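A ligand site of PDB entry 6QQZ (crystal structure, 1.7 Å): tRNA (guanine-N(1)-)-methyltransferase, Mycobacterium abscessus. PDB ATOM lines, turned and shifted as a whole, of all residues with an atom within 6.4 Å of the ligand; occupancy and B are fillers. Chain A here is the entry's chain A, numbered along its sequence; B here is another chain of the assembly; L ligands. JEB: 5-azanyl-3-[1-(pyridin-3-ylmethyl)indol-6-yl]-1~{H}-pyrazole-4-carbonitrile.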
ATOM      1  N   VAL A  84      24.532 -21.670   3.221  1.00  0.00           N
ATOM      2  CA  VAL A  84      25.234 -22.144   2.035  1.00  0.00           C
ATOM      3  C   VAL A  84      24.693 -23.519   1.668  1.00  0.00           C
ATOM      4  O   VAL A  84      25.086 -24.510   2.269  1.00  0.00           O
ATOM      5  CB  VAL A  84      26.754 -22.255   2.259  1.00  0.00           C
ATOM      6  CG1 VAL A  84      27.443 -22.699   0.970  1.00  0.00           C
ATOM      7  CG2 VAL A  84      27.345 -20.921   2.766  1.00  0.00           C
ATOM      8  N   PRO A  85      23.778 -23.572   0.691  1.00  0.00           N
ATOM      9  CA  PRO A  85      23.300 -24.877   0.236  1.00  0.00           C
ATOM     10  C   PRO A  85      24.443 -25.705  -0.332  1.00  0.00           C
ATOM     11  O   PRO A  85      25.315 -25.152  -0.984  1.00  0.00           O
ATOM     12  CB  PRO A  85      22.277 -24.516  -0.864  1.00  0.00           C
ATOM     13  CG  PRO A  85      21.763 -23.148  -0.444  1.00  0.00           C
ATOM     14  CD  PRO A  85      23.012 -22.453   0.096  1.00  0.00           C
ATOM     15  N   THR A  86      24.432 -27.008  -0.072  1.00  0.00           N
ATOM     16  CA  THR A  86      25.471 -27.885  -0.595  1.00  0.00           C
ATOM     17  C   THR A  86      24.987 -29.306  -0.409  1.00  0.00           C
ATOM     18  O   THR A  86      24.370 -29.606   0.595  1.00  0.00           O
ATOM     19  CB  THR A  86      26.836 -27.665   0.111  1.00  0.00           C
ATOM     20  OG1 THR A  86      27.711 -28.778  -0.141  1.00  0.00           O
ATOM     21  CG2 THR A  86      26.671 -27.460   1.613  1.00  0.00           C
ATOM     22  N   PRO A  87      25.272 -30.165  -1.378  1.00  0.00           N
ATOM     23  CA  PRO A  87      24.847 -31.557  -1.202  1.00  0.00           C
ATOM     24  C   PRO A  87      25.560 -32.239  -0.022  1.00  0.00           C
ATOM     25  O   PRO A  87      25.083 -33.300   0.430  1.00  0.00           O
ATOM     26  CB  PRO A  87      25.212 -32.217  -2.536  1.00  0.00           C
ATOM     27  CG  PRO A  87      26.215 -31.338  -3.145  1.00  0.00           C
ATOM     28  CD  PRO A  87      25.984 -29.938  -2.646  1.00  0.00           C
ATOM     29  N   ALA A  88      26.630 -31.632   0.472  1.00  0.00           N
ATOM     30  CA  ALA A  88      27.387 -32.164   1.609  1.00  0.00           C
ATOM     31  C   ALA A  88      27.006 -31.480   2.919  1.00  0.00           C
ATOM     32  O   ALA A  88      27.708 -31.620   3.926  1.00  0.00           O
ATOM     33  CB  ALA A  88      28.886 -32.023   1.349  1.00  0.00           C
ATOM     34  N   CYS A 110      24.373 -19.045  -3.232  1.00  0.00           N
ATOM     35  CA  CYS A 110      24.066 -20.150  -4.153  1.00  0.00           C
ATOM     36  C   CYS A 110      25.246 -20.490  -5.037  1.00  0.00           C
ATOM     37  O   CYS A 110      25.681 -19.658  -5.841  1.00  0.00           O
ATOM     38  CB  CYS A 110      22.871 -19.814  -5.040  1.00  0.00           C
ATOM     39  SG  CYS A 110      21.345 -19.483  -4.131  1.00  0.00           S
ATOM     40  N   GLY A 111      25.743 -21.715  -4.912  1.00  0.00           N
ATOM     41  CA  GLY A 111      26.808 -22.149  -5.785  1.00  0.00           C
ATOM     42  C   GLY A 111      26.301 -22.798  -7.052  1.00  0.00           C
ATOM     43  O   GLY A 111      25.108 -23.128  -7.177  1.00  0.00           O
ATOM     44  N   ARG A 112      27.233 -23.003  -7.976  1.00  0.00           N
ATOM     45  CA  ARG A 112      27.036 -23.788  -9.191  1.00  0.00           C
ATOM     46  C   ARG A 112      28.306 -24.604  -9.398  1.00  0.00           C
ATOM     47  O   ARG A 112      29.233 -24.509  -8.596  1.00  0.00           O
ATOM     48  CB  ARG A 112      26.750 -22.878 -10.393  1.00  0.00           C
ATOM     49  CG  ARG A 112      25.320 -22.323 -10.425  1.00  0.00           C
ATOM     50  CD  ARG A 112      24.407 -23.311 -11.186  1.00  0.00           C
ATOM     51  NE  ARG A 112      23.007 -23.194 -10.784  1.00  0.00           N
ATOM     52  CZ  ARG A 112      22.017 -23.800 -11.405  1.00  0.00           C
ATOM     53  NH1 ARG A 112      22.270 -24.556 -12.483  1.00  0.00           N
ATOM     54  NH2 ARG A 112      20.762 -23.649 -10.974  1.00  0.00           N
ATOM     55  N   TYR A 113      28.347 -25.405 -10.470  1.00  0.00           N
ATOM     56  CA  TYR A 113      29.494 -26.263 -10.762  1.00  0.00           C
ATOM     57  C   TYR A 113      29.764 -27.219  -9.607  1.00  0.00           C
ATOM     58  O   TYR A 113      28.831 -27.863  -9.113  1.00  0.00           O
ATOM     59  CB  TYR A 113      30.729 -25.414 -11.070  1.00  0.00           C
ATOM     60  CG  TYR A 113      30.454 -24.295 -12.046  1.00  0.00           C
ATOM     61  CD1 TYR A 113      30.209 -24.579 -13.379  1.00  0.00           C
ATOM     62  CD2 TYR A 113      30.425 -22.970 -11.642  1.00  0.00           C
ATOM     63  CE1 TYR A 113      29.961 -23.569 -14.289  1.00  0.00           C
ATOM     64  CE2 TYR A 113      30.171 -21.953 -12.534  1.00  0.00           C
ATOM     65  CZ  TYR A 113      29.935 -22.262 -13.856  1.00  0.00           C
ATOM     66  OH  TYR A 113      29.675 -21.245 -14.761  1.00  0.00           O
ATOM     67  N   GLU A 114      31.006 -27.355  -9.163  1.00  0.00           N
ATOM     68  CA  GLU A 114      31.280 -28.292  -8.080  1.00  0.00           C
ATOM     69  C   GLU A 114      31.051 -27.659  -6.712  1.00  0.00           C
ATOM     70  O   GLU A 114      31.092 -28.339  -5.690  1.00  0.00           O
ATOM     71  CB  GLU A 114      32.702 -28.846  -8.183  1.00  0.00           C
ATOM     72  CG  GLU A 114      32.930 -29.636  -9.458  1.00  0.00           C
ATOM     73  CD  GLU A 114      31.945 -30.793  -9.595  1.00  0.00           C
ATOM     74  OE1 GLU A 114      31.019 -30.701 -10.444  1.00  0.00           O
ATOM     75  OE2 GLU A 114      32.091 -31.781  -8.849  1.00  0.00           O
ATOM     76  N   GLY A 115      30.777 -26.358  -6.695  1.00  0.00           N
ATOM     77  CA  GLY A 115      30.536 -25.654  -5.453  1.00  0.00           C
ATOM     78  C   GLY A 115      31.482 -24.477  -5.291  1.00  0.00           C
ATOM     79  O   GLY A 115      32.162 -24.092  -6.222  1.00  0.00           O
ATOM     80  N   ILE A 116      31.542 -23.943  -4.078  1.00  0.00           N
ATOM     81  CA  ILE A 116      32.345 -22.760  -3.770  1.00  0.00           C
ATOM     82  C   ILE A 116      33.610 -23.174  -3.044  1.00  0.00           C
ATOM     83  O   ILE A 116      33.558 -24.027  -2.166  1.00  0.00           O
ATOM     84  CB  ILE A 116      31.553 -21.779  -2.884  1.00  0.00           C
ATOM     85  CG1 ILE A 116      30.176 -21.487  -3.500  1.00  0.00           C
ATOM     86  CG2 ILE A 116      32.353 -20.496  -2.574  1.00  0.00           C
ATOM     87  CD1 ILE A 116      29.299 -20.595  -2.639  1.00  0.00           C
ATOM     88  N   VAL A 133      24.051 -26.416   4.501  1.00  0.00           N
ATOM     89  CA  VAL A 133      22.891 -27.309   4.662  1.00  0.00           C
ATOM     90  C   VAL A 133      22.497 -27.945   3.354  1.00  0.00           C
ATOM     91  O   VAL A 133      22.750 -27.368   2.290  1.00  0.00           O
ATOM     92  CB  VAL A 133      21.644 -26.553   5.205  1.00  0.00           C
ATOM     93  CG1 VAL A 133      21.878 -26.062   6.636  1.00  0.00           C
ATOM     94  CG2 VAL A 133      21.266 -25.362   4.282  1.00  0.00           C
ATOM     95  N   SER A 134      21.849 -29.101   3.433  1.00  0.00           N
ATOM     96  CA  SER A 134      21.286 -29.767   2.252  1.00  0.00           C
ATOM     97  C   SER A 134      19.783 -29.976   2.421  1.00  0.00           C
ATOM     98  O   SER A 134      19.338 -30.375   3.506  1.00  0.00           O
ATOM     99  CB  SER A 134      21.968 -31.118   2.006  1.00  0.00           C
ATOM    100  OG  SER A 134      21.218 -31.913   1.098  1.00  0.00           O
ATOM    101  N   ILE A 135      18.998 -29.748   1.358  1.00  0.00           N
ATOM    102  CA  ILE A 135      17.539 -29.886   1.477  1.00  0.00           C
ATOM    103  C   ILE A 135      17.052 -31.315   1.233  1.00  0.00           C
ATOM    104  O   ILE A 135      15.867 -31.585   1.412  1.00  0.00           O
ATOM    105  CB  ILE A 135      16.773 -28.928   0.512  1.00  0.00           C
ATOM    106  CG1 ILE A 135      17.161 -29.161  -0.947  1.00  0.00           C
ATOM    107  CG2 ILE A 135      17.010 -27.472   0.902  1.00  0.00           C
ATOM    108  CD1 ILE A 135      16.071 -28.658  -1.949  1.00  0.00           C
ATOM    109  N   GLY A 136      17.945 -32.221   0.835  1.00  0.00           N
ATOM    110  CA  GLY A 136      17.525 -33.600   0.655  1.00  0.00           C
ATOM    111  C   GLY A 136      18.560 -34.478  -0.013  1.00  0.00           C
ATOM    112  O   GLY A 136      19.586 -33.998  -0.478  1.00  0.00           O
ATOM    113  N   ASP A 137      18.270 -35.779  -0.072  1.00  0.00           N
ATOM    114  CA  ASP A 137      19.263 -36.727  -0.545  1.00  0.00           C
ATOM    115  C   ASP A 137      19.159 -37.008  -2.039  1.00  0.00           C
ATOM    116  O   ASP A 137      18.897 -38.133  -2.464  1.00  0.00           O
ATOM    117  CB  ASP A 137      19.148 -38.039   0.245  1.00  0.00           C
ATOM    118  CG  ASP A 137      19.634 -37.878   1.667  1.00  0.00           C
ATOM    119  OD1 ASP A 137      20.432 -36.945   1.909  1.00  0.00           O
ATOM    120  OD2 ASP A 137      19.238 -38.683   2.531  1.00  0.00           O
ATOM    121  N   TYR A 138      19.369 -35.962  -2.823  1.00  0.00           N
ATOM    122  CA  TYR A 138      19.382 -36.000  -4.275  1.00  0.00           C
ATOM    123  C   TYR A 138      20.352 -34.910  -4.685  1.00  0.00           C
ATOM    124  O   TYR A 138      20.698 -34.059  -3.880  1.00  0.00           O
ATOM    125  CB  TYR A 138      17.999 -35.736  -4.874  1.00  0.00           C
ATOM    126  CG  TYR A 138      17.240 -34.725  -4.063  1.00  0.00           C
ATOM    127  CD1 TYR A 138      17.516 -33.350  -4.175  1.00  0.00           C
ATOM    128  CD2 TYR A 138      16.269 -35.130  -3.161  1.00  0.00           C
ATOM    129  CE1 TYR A 138      16.822 -32.431  -3.424  1.00  0.00           C
ATOM    130  CE2 TYR A 138      15.572 -34.220  -2.408  1.00  0.00           C
ATOM    131  CZ  TYR A 138      15.859 -32.874  -2.540  1.00  0.00           C
ATOM    132  OH  TYR A 138      15.169 -31.985  -1.766  1.00  0.00           O
ATOM    133  N   VAL A 139      20.738 -34.924  -5.959  1.00  0.00           N
ATOM    134  CA  VAL A 139      21.740 -33.992  -6.453  1.00  0.00           C
ATOM    135  C   VAL A 139      21.109 -32.988  -7.406  1.00  0.00           C
ATOM    136  O   VAL A 139      20.392 -33.372  -8.321  1.00  0.00           O
ATOM    137  CB  VAL A 139      22.876 -34.734  -7.171  1.00  0.00           C
ATOM    138  CG1 VAL A 139      23.922 -33.731  -7.660  1.00  0.00           C
ATOM    139  CG2 VAL A 139      23.487 -35.780  -6.256  1.00  0.00           C
ATOM    140  N   LEU A 140      21.355 -31.702  -7.159  1.00  0.00           N
ATOM    141  CA  LEU A 140      20.867 -30.644  -8.035  1.00  0.00           C
ATOM    142  C   LEU A 140      22.036 -30.057  -8.815  1.00  0.00           C
ATOM    143  O   LEU A 140      23.185 -30.459  -8.608  1.00  0.00           O
ATOM    144  CB  LEU A 140      20.185 -29.553  -7.211  1.00  0.00           C
ATOM    145  CG  LEU A 140      19.057 -30.047  -6.303  1.00  0.00           C
ATOM    146  CD1 LEU A 140      18.670 -28.980  -5.314  1.00  0.00           C
ATOM    147  CD2 LEU A 140      17.836 -30.455  -7.132  1.00  0.00           C
ATOM    148  N   ASN A 141      21.760 -29.084  -9.690  1.00  0.00           N
ATOM    149  CA  ASN A 141      22.829 -28.445 -10.466  1.00  0.00           C
ATOM    150  C   ASN A 141      23.467 -27.274  -9.725  1.00  0.00           C
ATOM    151  O   ASN A 141      24.544 -26.779 -10.111  1.00  0.00           O
ATOM    152  CB  ASN A 141      22.284 -27.923 -11.802  1.00  0.00           C
ATOM    153  CG  ASN A 141      21.972 -29.034 -12.768  1.00  0.00           C
ATOM    154  OD1 ASN A 141      22.702 -30.018 -12.857  1.00  0.00           O
ATOM    155  ND2 ASN A 141      20.874 -28.885 -13.496  1.00  0.00           N
ATOM    156  N   GLY A 142      22.804 -26.807  -8.678  1.00  0.00           N
ATOM    157  CA  GLY A 142      23.321 -25.657  -7.962  1.00  0.00           C
ATOM    158  C   GLY A 142      22.406 -25.321  -6.807  1.00  0.00           C
ATOM    159  O   GLY A 142      21.424 -26.030  -6.554  1.00  0.00           O
ATOM    160  N   GLY A 143      22.729 -24.240  -6.115  1.00  0.00           N
ATOM    161  CA  GLY A 143      22.031 -23.881  -4.892  1.00  0.00           C
ATOM    162  C   GLY A 143      20.680 -23.190  -5.028  1.00  0.00           C
ATOM    163  O   GLY A 143      19.974 -23.043  -4.039  1.00  0.00           O
ATOM    164  N   GLU A 144      20.308 -22.783  -6.246  1.00  0.00           N
ATOM    165  CA  GLU A 144      19.130 -21.902  -6.402  1.00  0.00           C
ATOM    166  C   GLU A 144      17.813 -22.574  -6.012  1.00  0.00           C
ATOM    167  O   GLU A 144      16.978 -21.968  -5.323  1.00  0.00           O
ATOM    168  CB  GLU A 144      19.039 -21.382  -7.833  1.00  0.00           C
ATOM    169  CG  GLU A 144      20.104 -20.341  -8.184  1.00  0.00           C
ATOM    170  CD  GLU A 144      21.491 -20.933  -8.464  1.00  0.00           C
ATOM    171  OE1 GLU A 144      21.612 -22.168  -8.577  1.00  0.00           O
ATOM    172  OE2 GLU A 144      22.448 -20.133  -8.622  1.00  0.00           O
ATOM    173  N   ALA A 146      17.448 -24.978  -3.975  1.00  0.00           N
ATOM    174  CA  ALA A 146      17.519 -25.137  -2.520  1.00  0.00           C
ATOM    175  C   ALA A 146      17.181 -23.842  -1.806  1.00  0.00           C
ATOM    176  O   ALA A 146      16.514 -23.866  -0.773  1.00  0.00           O
ATOM    177  CB  ALA A 146      18.921 -25.624  -2.099  1.00  0.00           C
ATOM    178  N   ILE A 150      14.275 -23.302   0.974  1.00  0.00           N
ATOM    179  CA  ILE A 150      14.598 -22.768   2.290  1.00  0.00           C
ATOM    180  C   ILE A 150      13.811 -21.489   2.565  1.00  0.00           C
ATOM    181  O   ILE A 150      13.246 -21.318   3.640  1.00  0.00           O
ATOM    182  CB  ILE A 150      16.103 -22.510   2.404  1.00  0.00           C
ATOM    183  CG1 ILE A 150      16.851 -23.853   2.422  1.00  0.00           C
ATOM    184  CG2 ILE A 150      16.409 -21.704   3.673  1.00  0.00           C
ATOM    185  CD1 ILE A 150      18.361 -23.748   2.166  1.00  0.00           C
ATOM    186  N   ARG B 156      18.753 -33.689 -15.090  1.00  0.00           N
ATOM    187  CA  ARG B 156      20.195 -33.765 -15.225  1.00  0.00           C
ATOM    188  C   ARG B 156      20.710 -35.212 -15.399  1.00  0.00           C
ATOM    189  O   ARG B 156      21.870 -35.417 -15.736  1.00  0.00           O
ATOM    190  CB  ARG B 156      20.876 -33.081 -14.041  1.00  0.00           C
ATOM    191  CG  ARG B 156      20.642 -33.736 -12.692  1.00  0.00           C
ATOM    192  CD  ARG B 156      21.168 -32.828 -11.588  1.00  0.00           C
ATOM    193  NE  ARG B 156      22.619 -32.661 -11.619  1.00  0.00           N
ATOM    194  CZ  ARG B 156      23.492 -33.603 -11.263  1.00  0.00           C
ATOM    195  NH1 ARG B 156      23.069 -34.790 -10.841  1.00  0.00           N
ATOM    196  NH2 ARG B 156      24.790 -33.346 -11.320  1.00  0.00           N
ATOM    197  N   GLU B 182      30.316 -35.328  -0.333  1.00  0.00           N
ATOM    198  CA  GLU B 182      31.488 -34.826  -1.030  1.00  0.00           C
ATOM    199  C   GLU B 182      32.328 -33.944  -0.106  1.00  0.00           C
ATOM    200  O   GLU B 182      31.793 -33.300   0.809  1.00  0.00           O
ATOM    201  CB  GLU B 182      31.076 -34.084  -2.300  1.00  0.00           C
ATOM    202  CG  GLU B 182      31.414 -34.893  -3.553  1.00  0.00           C
ATOM    203  CD  GLU B 182      30.929 -34.256  -4.838  1.00  0.00           C
ATOM    204  OE1 GLU B 182      31.425 -33.162  -5.183  1.00  0.00           O
ATOM    205  OE2 GLU B 182      30.061 -34.864  -5.503  1.00  0.00           O
HETATM  206  C10 JEB L   1      23.513 -27.270  -3.526  1.00  0.00           C
HETATM  207  C13 JEB L   1      25.082 -27.819  -5.854  1.00  0.00           C
HETATM  208  C17 JEB L   1      26.933 -30.152  -7.372  1.00  0.00           C
HETATM  209  C20 JEB L   1      28.454 -32.232  -6.423  1.00  0.00           C
HETATM  210  C21 JEB L   1      27.450 -32.517  -7.369  1.00  0.00           C
HETATM  211  C22 JEB L   1      26.663 -31.439  -7.871  1.00  0.00           C
HETATM  212  C24 JEB L   1      26.314 -25.927  -5.816  1.00  0.00           C
HETATM  213  N01 JEB L   1      20.128 -31.375  -1.659  1.00  0.00           N
HETATM  214  C02 JEB L   1      20.987 -30.900  -2.668  1.00  0.00           C
HETATM  215  N03 JEB L   1      21.390 -31.516  -3.726  1.00  0.00           N
HETATM  216  N04 JEB L   1      22.251 -30.680  -4.404  1.00  0.00           N
HETATM  217  C05 JEB L   1      22.350 -29.543  -3.786  1.00  0.00           C
HETATM  218  C06 JEB L   1      21.627 -29.625  -2.643  1.00  0.00           C
HETATM  219  C07 JEB L   1      21.378 -28.636  -1.537  1.00  0.00           C
HETATM  220  N08 JEB L   1      21.167 -27.913  -0.677  1.00  0.00           N
HETATM  221  C09 JEB L   1      23.312 -28.474  -4.269  1.00  0.00           C
HETATM  222  C11 JEB L   1      24.480 -26.336  -3.965  1.00  0.00           C
HETATM  223  C12 JEB L   1      25.277 -26.627  -5.131  1.00  0.00           C
HETATM  224  C14 JEB L   1      24.112 -28.783  -5.406  1.00  0.00           C
HETATM  225  N15 JEB L   1      25.973 -27.846  -6.915  1.00  0.00           N
HETATM  226  C16 JEB L   1      26.081 -28.945  -7.915  1.00  0.00           C
HETATM  227  C18 JEB L   1      27.982 -29.958  -6.414  1.00  0.00           C
HETATM  228  N19 JEB L   1      28.684 -30.984  -5.992  1.00  0.00           N
HETATM  229  C23 JEB L   1      26.720 -26.718  -6.929  1.00  0.00           C
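O of Tyr 138 is in hydrogen-bond range of N03 of the ligand (2.6 Å).
N01 of the ligand lies within hydrogen-bond range of O of Gly 136, at 2.9 Å.
N01 of the ligand is in hydrogen-bond range of OG of Ser 134.
The backbone NH (N) of Leu 140 is in hydrogen-bond range of a nitrogen (N04) of the ligand (3.1 Å).
N of Thr 86 is in hydrogen-bond range of N08 of the ligand (3.4 Å).
N08 of the ligand lies within hydrogen-bond range of N of Ile 135, 3.5 Å away.
The backbone carbonyl oxygen of Ile 135 is in hydrogen-bond range of the side-chain hydroxyl of Tyr 138, 3.3 Å away.
The side-chain hydroxyl (OG) of Ser 134 lies within hydrogen-bond range of the backbone carbonyl oxygen (O) of Gly 136 (3.1 Å).
The backbone carbonyl oxygen of Gly 111 lies within hydrogen-bond range of the backbone NH of Gly 143, 2.8 Å away.
The backbone NH (N) of Thr 86 is in hydrogen-bond range of the backbone carbonyl oxygen (O) of Val 133 (2.9 Å).
The backbone carbonyl oxygen of Val 84 lies within hydrogen-bond range of the backbone NH of Val 133, 3.1 Å away.
OG1 of Thr 86 sits close to N of Ala 88.
The side-chain amide oxygen (OD1) of Asn 141 is in hydrogen-bond range of the guanidinium group (NE) of Arg 156 of chain B (2.9 Å).
The side-chain carboxylate (OE1) of Glu 144 is in salt-bridge range of the guanidinium group (NE) of Arg 112 (2.8 Å).
N08 of the ligand lies close to O of Val 133 (3.4 Å).
O of Pro 85 touches C11 of the ligand, at 3.3 Å.
CD of Pro 87 touches C09 of the ligand, 3.5 Å away.
Gly 111 touches the ligand.
Arg 112 touches the ligand.
Tyr 113 touches the ligand (O to C16, 3.2 Å).
Glu 114 touches the ligand (O to C18, 3.6 Å).
Val 139 touches the ligand.
Asn 141 touches the ligand (O to C16, 3.4 Å).
Gly 142 touches the ligand (CA to C13, 3.5 Å).
Gly 143 touches the ligand (N to C11, 3.5 Å).
Ala 146 touches the ligand (CB to N08, 3.5 Å).
Glu 182 of chain B touches the ligand (OE2 to C20, 3.2 Å).
Hydrophobic or aromatic side chains that line the ligand: Pro 85, Pro 87, Ile 135, Tyr 138, Val 139, Leu 140 and Ala 146.
19 residues have an atom within 4 Å of the ligand: Pro 85, Thr 86, Pro 87, Gly 111, Arg 112, Tyr 113, Glu 114, Val 133, Ser 134, Ile 135, Gly 136, Tyr 138, Val 139, Leu 140, Asn 141, Gly 142, Gly 143, Ala 146 and Glu 182 of chain B.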
